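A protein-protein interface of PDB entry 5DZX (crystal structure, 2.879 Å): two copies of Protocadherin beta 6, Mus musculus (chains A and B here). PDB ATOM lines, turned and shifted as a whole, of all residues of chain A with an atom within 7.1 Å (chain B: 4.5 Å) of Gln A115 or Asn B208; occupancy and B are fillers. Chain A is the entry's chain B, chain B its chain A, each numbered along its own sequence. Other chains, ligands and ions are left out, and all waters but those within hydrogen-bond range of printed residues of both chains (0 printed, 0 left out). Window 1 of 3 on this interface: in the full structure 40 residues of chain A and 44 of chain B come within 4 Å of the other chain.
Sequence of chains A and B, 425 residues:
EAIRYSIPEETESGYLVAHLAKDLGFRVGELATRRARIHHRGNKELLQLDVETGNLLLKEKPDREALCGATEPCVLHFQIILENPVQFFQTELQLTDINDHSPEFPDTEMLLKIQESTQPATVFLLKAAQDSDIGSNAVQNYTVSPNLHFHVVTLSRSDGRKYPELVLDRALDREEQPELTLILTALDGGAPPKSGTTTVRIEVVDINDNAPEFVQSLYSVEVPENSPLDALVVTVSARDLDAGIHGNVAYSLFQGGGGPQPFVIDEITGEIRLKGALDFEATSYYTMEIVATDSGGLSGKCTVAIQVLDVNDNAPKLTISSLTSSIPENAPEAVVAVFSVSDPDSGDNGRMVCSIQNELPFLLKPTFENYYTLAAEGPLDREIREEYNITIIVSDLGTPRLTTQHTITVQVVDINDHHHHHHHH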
ATOM      1  N   LYS A 113      -5.964  22.970 -23.833  1.00  0.00           N
ATOM      2  CA  LYS A 113      -6.801  23.672 -22.876  1.00  0.00           C
ATOM      3  C   LYS A 113      -6.884  22.861 -21.592  1.00  0.00           C
ATOM      4  O   LYS A 113      -7.493  21.797 -21.561  1.00  0.00           O
ATOM      5  CB  LYS A 113      -8.195  23.925 -23.453  1.00  0.00           C
ATOM      6  CG  LYS A 113      -8.203  24.885 -24.633  1.00  0.00           C
ATOM      7  CD  LYS A 113      -9.609  25.374 -24.954  1.00  0.00           C
ATOM      8  CE  LYS A 113     -10.439  24.315 -25.657  1.00  0.00           C
ATOM      9  NZ  LYS A 113     -11.759  24.856 -26.092  1.00  0.00           N
ATOM     10  N   ILE A 114      -6.256  23.369 -20.536  1.00  0.00           N
ATOM     11  CA  ILE A 114      -6.231  22.689 -19.246  1.00  0.00           C
ATOM     12  C   ILE A 114      -6.850  23.570 -18.168  1.00  0.00           C
ATOM     13  O   ILE A 114      -6.331  24.645 -17.872  1.00  0.00           O
ATOM     14  CB  ILE A 114      -4.793  22.317 -18.836  1.00  0.00           C
ATOM     15  CG1 ILE A 114      -4.098  21.548 -19.961  1.00  0.00           C
ATOM     16  CG2 ILE A 114      -4.796  21.524 -17.537  1.00  0.00           C
ATOM     17  CD1 ILE A 114      -2.688  21.115 -19.627  1.00  0.00           C
ATOM     18  N   GLN A 115      -7.956  23.116 -17.583  1.00  0.00           N
ATOM     19  CA  GLN A 115      -8.675  23.924 -16.603  1.00  0.00           C
ATOM     20  C   GLN A 115      -7.825  24.205 -15.370  1.00  0.00           C
ATOM     21  O   GLN A 115      -6.945  23.422 -15.010  1.00  0.00           O
ATOM     22  CB  GLN A 115      -9.986  23.248 -16.191  1.00  0.00           C
ATOM     23  CG  GLN A 115      -9.818  21.950 -15.425  1.00  0.00           C
ATOM     24  CD  GLN A 115     -11.147  21.296 -15.101  1.00  0.00           C
ATOM     25  OE1 GLN A 115     -12.186  21.674 -15.645  1.00  0.00           O
ATOM     26  NE2 GLN A 115     -11.123  20.313 -14.207  1.00  0.00           N
ATOM     27  N   GLU A 116      -8.105  25.340 -14.738  1.00  0.00           N
ATOM     28  CA  GLU A 116      -7.380  25.797 -13.559  1.00  0.00           C
ATOM     29  C   GLU A 116      -7.460  24.782 -12.418  1.00  0.00           C
ATOM     30  O   GLU A 116      -6.504  24.611 -11.662  1.00  0.00           O
ATOM     31  CB  GLU A 116      -7.943  27.151 -13.113  1.00  0.00           C
ATOM     32  CG  GLU A 116      -7.310  27.763 -11.874  1.00  0.00           C
ATOM     33  CD  GLU A 116      -8.034  29.024 -11.422  1.00  0.00           C
ATOM     34  OE1 GLU A 116      -9.005  29.428 -12.097  1.00  0.00           O
ATOM     35  OE2 GLU A 116      -7.630  29.611 -10.396  1.00  0.00           O
ATOM     36  N   SER A 117      -8.588  24.080 -12.330  1.00  0.00           N
ATOM     37  CA  SER A 117      -8.836  23.149 -11.230  1.00  0.00           C
ATOM     38  C   SER A 117      -8.270  21.756 -11.478  1.00  0.00           C
ATOM     39  O   SER A 117      -8.711  20.783 -10.864  1.00  0.00           O
ATOM     40  CB  SER A 117     -10.338  23.030 -10.968  1.00  0.00           C
ATOM     41  OG  SER A 117     -11.019  22.581 -12.128  1.00  0.00           O
ATOM     42  N   THR A 118      -7.290  21.660 -12.367  1.00  0.00           N
ATOM     43  CA  THR A 118      -6.695  20.370 -12.688  1.00  0.00           C
ATOM     44  C   THR A 118      -5.747  19.929 -11.580  1.00  0.00           C
ATOM     45  O   THR A 118      -4.869  20.686 -11.165  1.00  0.00           O
ATOM     46  CB  THR A 118      -5.939  20.414 -14.026  1.00  0.00           C
ATOM     47  OG1 THR A 118      -6.828  20.843 -15.064  1.00  0.00           O
ATOM     48  CG2 THR A 118      -5.391  19.038 -14.374  1.00  0.00           C
ATOM     49  N   GLN A 119      -5.940  18.707 -11.097  1.00  0.00           N
ATOM     50  CA  GLN A 119      -5.102  18.168 -10.035  1.00  0.00           C
ATOM     51  C   GLN A 119      -3.750  17.725 -10.577  1.00  0.00           C
ATOM     52  O   GLN A 119      -3.637  17.363 -11.748  1.00  0.00           O
ATOM     53  CB  GLN A 119      -5.806  17.005  -9.336  1.00  0.00           C
ATOM     54  CG  GLN A 119      -7.069  17.415  -8.601  1.00  0.00           C
ATOM     55  CD  GLN A 119      -7.737  16.251  -7.905  1.00  0.00           C
ATOM     56  OE1 GLN A 119      -7.328  15.102  -8.065  1.00  0.00           O
ATOM     57  NE2 GLN A 119      -8.767  16.544  -7.119  1.00  0.00           N
ATOM     58  N   PHE A 124      -1.185  14.166 -19.768  1.00  0.00           N
ATOM     59  CA  PHE A 124      -1.753  14.573 -21.047  1.00  0.00           C
ATOM     60  C   PHE A 124      -0.955  13.975 -22.200  1.00  0.00           C
ATOM     61  O   PHE A 124       0.261  13.816 -22.105  1.00  0.00           O
ATOM     62  CB  PHE A 124      -1.789  16.096 -21.158  1.00  0.00           C
ATOM     63  CG  PHE A 124      -2.614  16.754 -20.094  1.00  0.00           C
ATOM     64  CD1 PHE A 124      -3.939  17.081 -20.332  1.00  0.00           C
ATOM     65  CD2 PHE A 124      -2.073  17.034 -18.850  1.00  0.00           C
ATOM     66  CE1 PHE A 124      -4.705  17.682 -19.353  1.00  0.00           C
ATOM     67  CE2 PHE A 124      -2.835  17.633 -17.866  1.00  0.00           C
ATOM     68  CZ  PHE A 124      -4.153  17.958 -18.118  1.00  0.00           C
ATOM     69  N   LEU A 168       2.017  16.762 -14.973  1.00  0.00           N
ATOM     70  CA  LEU A 168       1.893  17.956 -14.146  1.00  0.00           C
ATOM     71  C   LEU A 168       2.258  17.691 -12.686  1.00  0.00           C
ATOM     72  O   LEU A 168       1.717  16.784 -12.056  1.00  0.00           O
ATOM     73  CB  LEU A 168       0.470  18.503 -14.234  1.00  0.00           C
ATOM     74  CG  LEU A 168       0.227  19.810 -13.486  1.00  0.00           C
ATOM     75  CD1 LEU A 168       1.175  20.880 -13.996  1.00  0.00           C
ATOM     76  CD2 LEU A 168      -1.220  20.241 -13.641  1.00  0.00           C
ATOM     77  N   LEU A 172      -2.116  24.466 -11.094  1.00  0.00           N
ATOM     78  CA  LEU A 172      -2.170  25.647 -11.948  1.00  0.00           C
ATOM     79  C   LEU A 172      -3.115  26.713 -11.411  1.00  0.00           C
ATOM     80  O   LEU A 172      -4.126  26.405 -10.780  1.00  0.00           O
ATOM     81  CB  LEU A 172      -2.596  25.259 -13.366  1.00  0.00           C
ATOM     82  CG  LEU A 172      -1.688  24.301 -14.137  1.00  0.00           C
ATOM     83  CD1 LEU A 172      -2.321  23.921 -15.468  1.00  0.00           C
ATOM     84  CD2 LEU A 172      -0.313  24.911 -14.348  1.00  0.00           C
ATOM     85  N   ASP A 173      -2.780  27.970 -11.678  1.00  0.00           N
ATOM     86  CA  ASP A 173      -3.626  29.093 -11.297  1.00  0.00           C
ATOM     87  C   ASP A 173      -3.680  30.098 -12.443  1.00  0.00           C
ATOM     88  O   ASP A 173      -2.645  30.546 -12.935  1.00  0.00           O
ATOM     89  CB  ASP A 173      -3.106  29.758 -10.021  1.00  0.00           C
ATOM     90  CG  ASP A 173      -4.224  30.271  -9.135  1.00  0.00           C
ATOM     91  OD1 ASP A 173      -5.276  29.600  -9.072  1.00  0.00           O
ATOM     92  OD2 ASP A 173      -4.050  31.335  -8.501  1.00  0.00           O
ATOM     93  N   GLU A 203      -3.425  26.533 -22.504  1.00  0.00           N
ATOM     94  CA  GLU A 203      -4.384  27.567 -22.140  1.00  0.00           C
ATOM     95  C   GLU A 203      -5.147  27.204 -20.872  1.00  0.00           C
ATOM     96  O   GLU A 203      -5.945  26.266 -20.865  1.00  0.00           O
ATOM     97  CB  GLU A 203      -5.364  27.803 -23.289  1.00  0.00           C
ATOM     98  CG  GLU A 203      -6.559  28.664 -22.926  1.00  0.00           C
ATOM     99  CD  GLU A 203      -7.523  28.828 -24.081  1.00  0.00           C
ATOM    100  OE1 GLU A 203      -7.144  28.490 -25.223  1.00  0.00           O
ATOM    101  OE2 GLU A 203      -8.662  29.284 -23.847  1.00  0.00           O
ATOM    102  N   VAL A 204      -4.919  27.961 -19.803  1.00  0.00           N
ATOM    103  CA  VAL A 204      -5.604  27.705 -18.545  1.00  0.00           C
ATOM    104  C   VAL A 204      -7.053  28.173 -18.632  1.00  0.00           C
ATOM    105  O   VAL A 204      -7.326  29.321 -18.988  1.00  0.00           O
ATOM    106  CB  VAL A 204      -4.905  28.400 -17.366  1.00  0.00           C
ATOM    107  CG1 VAL A 204      -5.507  27.932 -16.047  1.00  0.00           C
ATOM    108  CG2 VAL A 204      -3.414  28.117 -17.393  1.00  0.00           C
ATOM    109  N   VAL A 205      -7.978  27.274 -18.307  1.00  0.00           N
ATOM    110  CA  VAL A 205      -9.402  27.584 -18.363  1.00  0.00           C
ATOM    111  C   VAL A 205      -9.881  28.126 -17.022  1.00  0.00           C
ATOM    112  O   VAL A 205      -9.613  27.539 -15.974  1.00  0.00           O
ATOM    113  CB  VAL A 205     -10.237  26.345 -18.745  1.00  0.00           C
ATOM    114  CG1 VAL A 205     -11.725  26.666 -18.725  1.00  0.00           C
ATOM    115  CG2 VAL A 205      -9.814  25.822 -20.110  1.00  0.00           C
ATOM    116  N   ASP A 206     -10.592  29.247 -17.062  1.00  0.00           N
ATOM    117  CA  ASP A 206     -11.065  29.886 -15.841  1.00  0.00           C
ATOM    118  C   ASP A 206     -12.146  29.061 -15.164  1.00  0.00           C
ATOM    119  O   ASP A 206     -13.109  28.634 -15.802  1.00  0.00           O
ATOM    120  CB  ASP A 206     -11.593  31.293 -16.131  1.00  0.00           C
ATOM    121  CG  ASP A 206     -12.009  32.027 -14.872  1.00  0.00           C
ATOM    122  OD1 ASP A 206     -11.410  31.768 -13.806  1.00  0.00           O
ATOM    123  OD2 ASP A 206     -12.929  32.868 -14.949  1.00  0.00           O
ATOM    124  N   ILE A 207     -11.961  28.815 -13.873  1.00  0.00           N
ATOM    125  CA  ILE A 207     -12.981  28.163 -13.066  1.00  0.00           C
ATOM    126  C   ILE A 207     -13.301  29.042 -11.864  1.00  0.00           C
ATOM    127  O   ILE A 207     -12.579  29.998 -11.573  1.00  0.00           O
ATOM    128  CB  ILE A 207     -12.547  26.755 -12.606  1.00  0.00           C
ATOM    129  CG1 ILE A 207     -11.284  26.828 -11.748  1.00  0.00           C
ATOM    130  CG2 ILE A 207     -12.329  25.851 -13.812  1.00  0.00           C
ATOM    131  CD1 ILE A 207     -11.494  26.389 -10.321  1.00  0.00           C
ATOM    132  N   ILE B 207     -20.455  22.049 -12.959  1.00  0.00           N
ATOM    133  CA  ILE B 207     -19.015  22.231 -13.007  1.00  0.00           C
ATOM    134  C   ILE B 207     -18.388  21.058 -13.742  1.00  0.00           C
ATOM    135  O   ILE B 207     -19.044  20.049 -14.003  1.00  0.00           O
ATOM    136  CB  ILE B 207     -18.400  22.363 -11.602  1.00  0.00           C
ATOM    137  CG1 ILE B 207     -18.649  21.096 -10.785  1.00  0.00           C
ATOM    138  CG2 ILE B 207     -18.955  23.591 -10.895  1.00  0.00           C
ATOM    139  CD1 ILE B 207     -17.387  20.346 -10.440  1.00  0.00           C
ATOM    140  N   ASN B 208     -17.116  21.203 -14.088  1.00  0.00           N
ATOM    141  CA  ASN B 208     -16.431  20.194 -14.881  1.00  0.00           C
ATOM    142  C   ASN B 208     -15.762  19.126 -14.018  1.00  0.00           C
ATOM    143  O   ASN B 208     -14.602  19.266 -13.629  1.00  0.00           O
ATOM    144  CB  ASN B 208     -15.400  20.867 -15.782  1.00  0.00           C
ATOM    145  CG  ASN B 208     -15.107  20.064 -17.018  1.00  0.00           C
ATOM    146  OD1 ASN B 208     -15.935  19.271 -17.463  1.00  0.00           O
ATOM    147  ND2 ASN B 208     -13.926  20.265 -17.587  1.00  0.00           N
ATOM    148  N   ASP B 209     -16.491  18.049 -13.747  1.00  0.00           N
ATOM    149  CA  ASP B 209     -15.977  16.979 -12.897  1.00  0.00           C
ATOM    150  C   ASP B 209     -16.107  15.593 -13.532  1.00  0.00           C
ATOM    151  O   ASP B 209     -15.702  14.592 -12.940  1.00  0.00           O
ATOM    152  CB  ASP B 209     -16.687  17.007 -11.542  1.00  0.00           C
ATOM    153  CG  ASP B 209     -18.200  17.036 -11.672  1.00  0.00           C
ATOM    154  OD1 ASP B 209     -18.702  17.549 -12.694  1.00  0.00           O
ATOM    155  OD2 ASP B 209     -18.888  16.562 -10.745  1.00  0.00           O
ATOM    156  N   ASN B 210     -16.663  15.537 -14.739  1.00  0.00           N
ATOM    157  CA  ASN B 210     -16.797  14.272 -15.457  1.00  0.00           C
ATOM    158  C   ASN B 210     -16.094  14.283 -16.808  1.00  0.00           C
ATOM    159  O   ASN B 210     -16.444  15.061 -17.694  1.00  0.00           O
ATOM    160  CB  ASN B 210     -18.272  13.925 -15.651  1.00  0.00           C
ATOM    161  CG  ASN B 210     -18.962  13.577 -14.351  1.00  0.00           C
ATOM    162  OD1 ASN B 210     -18.351  13.013 -13.444  1.00  0.00           O
ATOM    163  ND2 ASN B 210     -20.239  13.917 -14.251  1.00  0.00           N
ATOM    164  N   ASP B 242     -21.541  16.046 -18.083  1.00  0.00           N
ATOM    165  CA  ASP B 242     -21.727  17.464 -17.795  1.00  0.00           C
ATOM    166  C   ASP B 242     -22.539  18.161 -18.885  1.00  0.00           C
ATOM    167  O   ASP B 242     -22.771  17.598 -19.956  1.00  0.00           O
ATOM    168  CB  ASP B 242     -20.371  18.149 -17.627  1.00  0.00           C
ATOM    169  CG  ASP B 242     -19.530  17.516 -16.535  1.00  0.00           C
ATOM    170  OD1 ASP B 242     -20.107  17.037 -15.537  1.00  0.00           O
ATOM    171  OD2 ASP B 242     -18.290  17.489 -16.678  1.00  0.00           O
ATOM    172  N   HIS B 246     -19.110  22.441 -20.487  1.00  0.00           N
ATOM    173  CA  HIS B 246     -18.462  21.320 -19.822  1.00  0.00           C
ATOM    174  C   HIS B 246     -18.916  19.996 -20.436  1.00  0.00           C
ATOM    175  O   HIS B 246     -18.401  18.932 -20.093  1.00  0.00           O
ATOM    176  CB  HIS B 246     -18.766  21.330 -18.320  1.00  0.00           C
ATOM    177  CG  HIS B 246     -18.612  22.673 -17.674  1.00  0.00           C
ATOM    178  ND1 HIS B 246     -17.386  23.275 -17.488  1.00  0.00           N
ATOM    179  CD2 HIS B 246     -19.530  23.522 -17.153  1.00  0.00           C
ATOM    180  CE1 HIS B 246     -17.556  24.440 -16.888  1.00  0.00           C
ATOM    181  NE2 HIS B 246     -18.848  24.614 -16.675  1.00  0.00           N
ATOM    182  N   ASP B 294     -12.415  17.612 -23.437  1.00  0.00           N
ATOM    183  CA  ASP B 294     -13.462  18.512 -22.984  1.00  0.00           C
ATOM    184  C   ASP B 294     -13.014  19.964 -23.141  1.00  0.00           C
ATOM    185  O   ASP B 294     -11.818  20.244 -23.265  1.00  0.00           O
ATOM    186  CB  ASP B 294     -13.828  18.213 -21.530  1.00  0.00           C
ATOM    187  CG  ASP B 294     -15.107  18.886 -21.108  1.00  0.00           C
ATOM    188  OD1 ASP B 294     -15.839  19.375 -21.993  1.00  0.00           O
ATOM    189  OD2 ASP B 294     -15.389  18.912 -19.895  1.00  0.00           O
ATOM    190  N   GLY B 296     -13.056  22.013 -20.928  1.00  0.00           N
ATOM    191  CA  GLY B 296     -12.392  22.344 -19.682  1.00  0.00           C
ATOM    192  C   GLY B 296     -10.982  21.783 -19.651  1.00  0.00           C
ATOM    193  O   GLY B 296     -10.042  22.459 -19.240  1.00  0.00           O
ATOM    194  N   GLY B 297     -10.831  20.545 -20.111  1.00  0.00           N
ATOM    195  CA  GLY B 297      -9.521  19.921 -20.168  1.00  0.00           C
ATOM    196  C   GLY B 297      -9.541  18.421 -19.958  1.00  0.00           C
ATOM    197  O   GLY B 297      -8.549  17.740 -20.220  1.00  0.00           O
ATOM    198  N   LEU B 298     -10.670  17.904 -19.485  1.00  0.00           N
ATOM    199  CA  LEU B 298     -10.802  16.472 -19.250  1.00  0.00           C
ATOM    200  C   LEU B 298     -10.817  15.715 -20.574  1.00  0.00           C
ATOM    201  O   LEU B 298     -11.374  16.189 -21.563  1.00  0.00           O
ATOM    202  CB  LEU B 298     -12.065  16.173 -18.447  1.00  0.00           C
ATOM    203  CG  LEU B 298     -12.208  16.925 -17.123  1.00  0.00           C
ATOM    204  CD1 LEU B 298     -13.440  16.443 -16.374  1.00  0.00           C
ATOM    205  CD2 LEU B 298     -10.955  16.793 -16.263  1.00  0.00           C
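The side-chain amide nitrogen (ND2) of Asn B208 sits at hydrogen-bond distance from the side-chain amide oxygen (OE1) of Gln A115.
The backbone carbonyl oxygen (O) of Gly B296 sits at hydrogen-bond distance from the backbone NH (N) of Gln A115, at 2.7 Å.
OD2 of Asp B242 lies close to OD1 of Asn B208 (3.1 Å).
The backbone NH of Ile A114 lies within hydrogen-bond range of the backbone carbonyl oxygen of Glu A203.
The backbone carbonyl oxygen (O) of Ile A114 lies within hydrogen-bond range of the backbone NH (N) of Val A205, 3.1 Å away.
The side-chain hydroxyl (OG) of Ser A117 lies within hydrogen-bond range of the side-chain amide nitrogen (NE2) of Gln A115 (3.1 Å).
O of Gln A115 is in hydrogen-bond range of OG1 of Thr A118 (2.6 Å).
The backbone NH (N) of Glu A116 lies within hydrogen-bond range of the backbone carbonyl oxygen (O) of Val A205, 2.9 Å away.
Lys A113 touches Gly B296 (O to O, 3.5 Å).
Lys A113 touches Gly B297 (O to CA, 3.1 Å).
Ile A114 touches Gly B296.
O of Gly B297 touches CE1 of Phe A124, 3.9 Å away.
Gly B296 touches Val A205 (O to CG2, 3.5 Å).
Printed residues of chain B within 4 Å of Ile A114: Gly B296 (3.5 Å).
Gln A115 touches just these residues of chain B: Asn B208 and Gly B296.
Thr A118 touches none of the printed residues of chain B.
Of the printed residues of chain B, Phe A124 touches Gly B297 (3.9 Å).
Printed residues of chain B within 4 Å of Val A205: Gly B296.
Of the printed residues of chain A, Gly B296 touches Lys A113, Ile A114, Gln A115 and Val A205.
Of the printed residues of chain A, Gly B297 touches Lys A113 and Phe A124.
Leu B298 touches none of the printed residues of chain A.
The nearest residue of chain A that does not touch Asn B208 is Ser A117 (5.1 Å).
The nearest printed residue of chain A that does not touch Gly B297 is Ile A114 (4.4 Å).
Printed residues of chain A that touch a printed residue of chain B: Lys A113, Ile A114, Gln A115, Phe A124 and Val A205.
Of the 10 printed residues of chain B, 3 touch a printed residue of chain A.
Printed residues of chain B that touch a printed residue of chain A: Asn B208, Gly B296 and Gly B297.
Among the printed residues, no Asp or Glu carboxylate lies within 4 Å of a Lys or Arg side-chain nitrogen of the other chain.
Position printed for both chains: 207.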
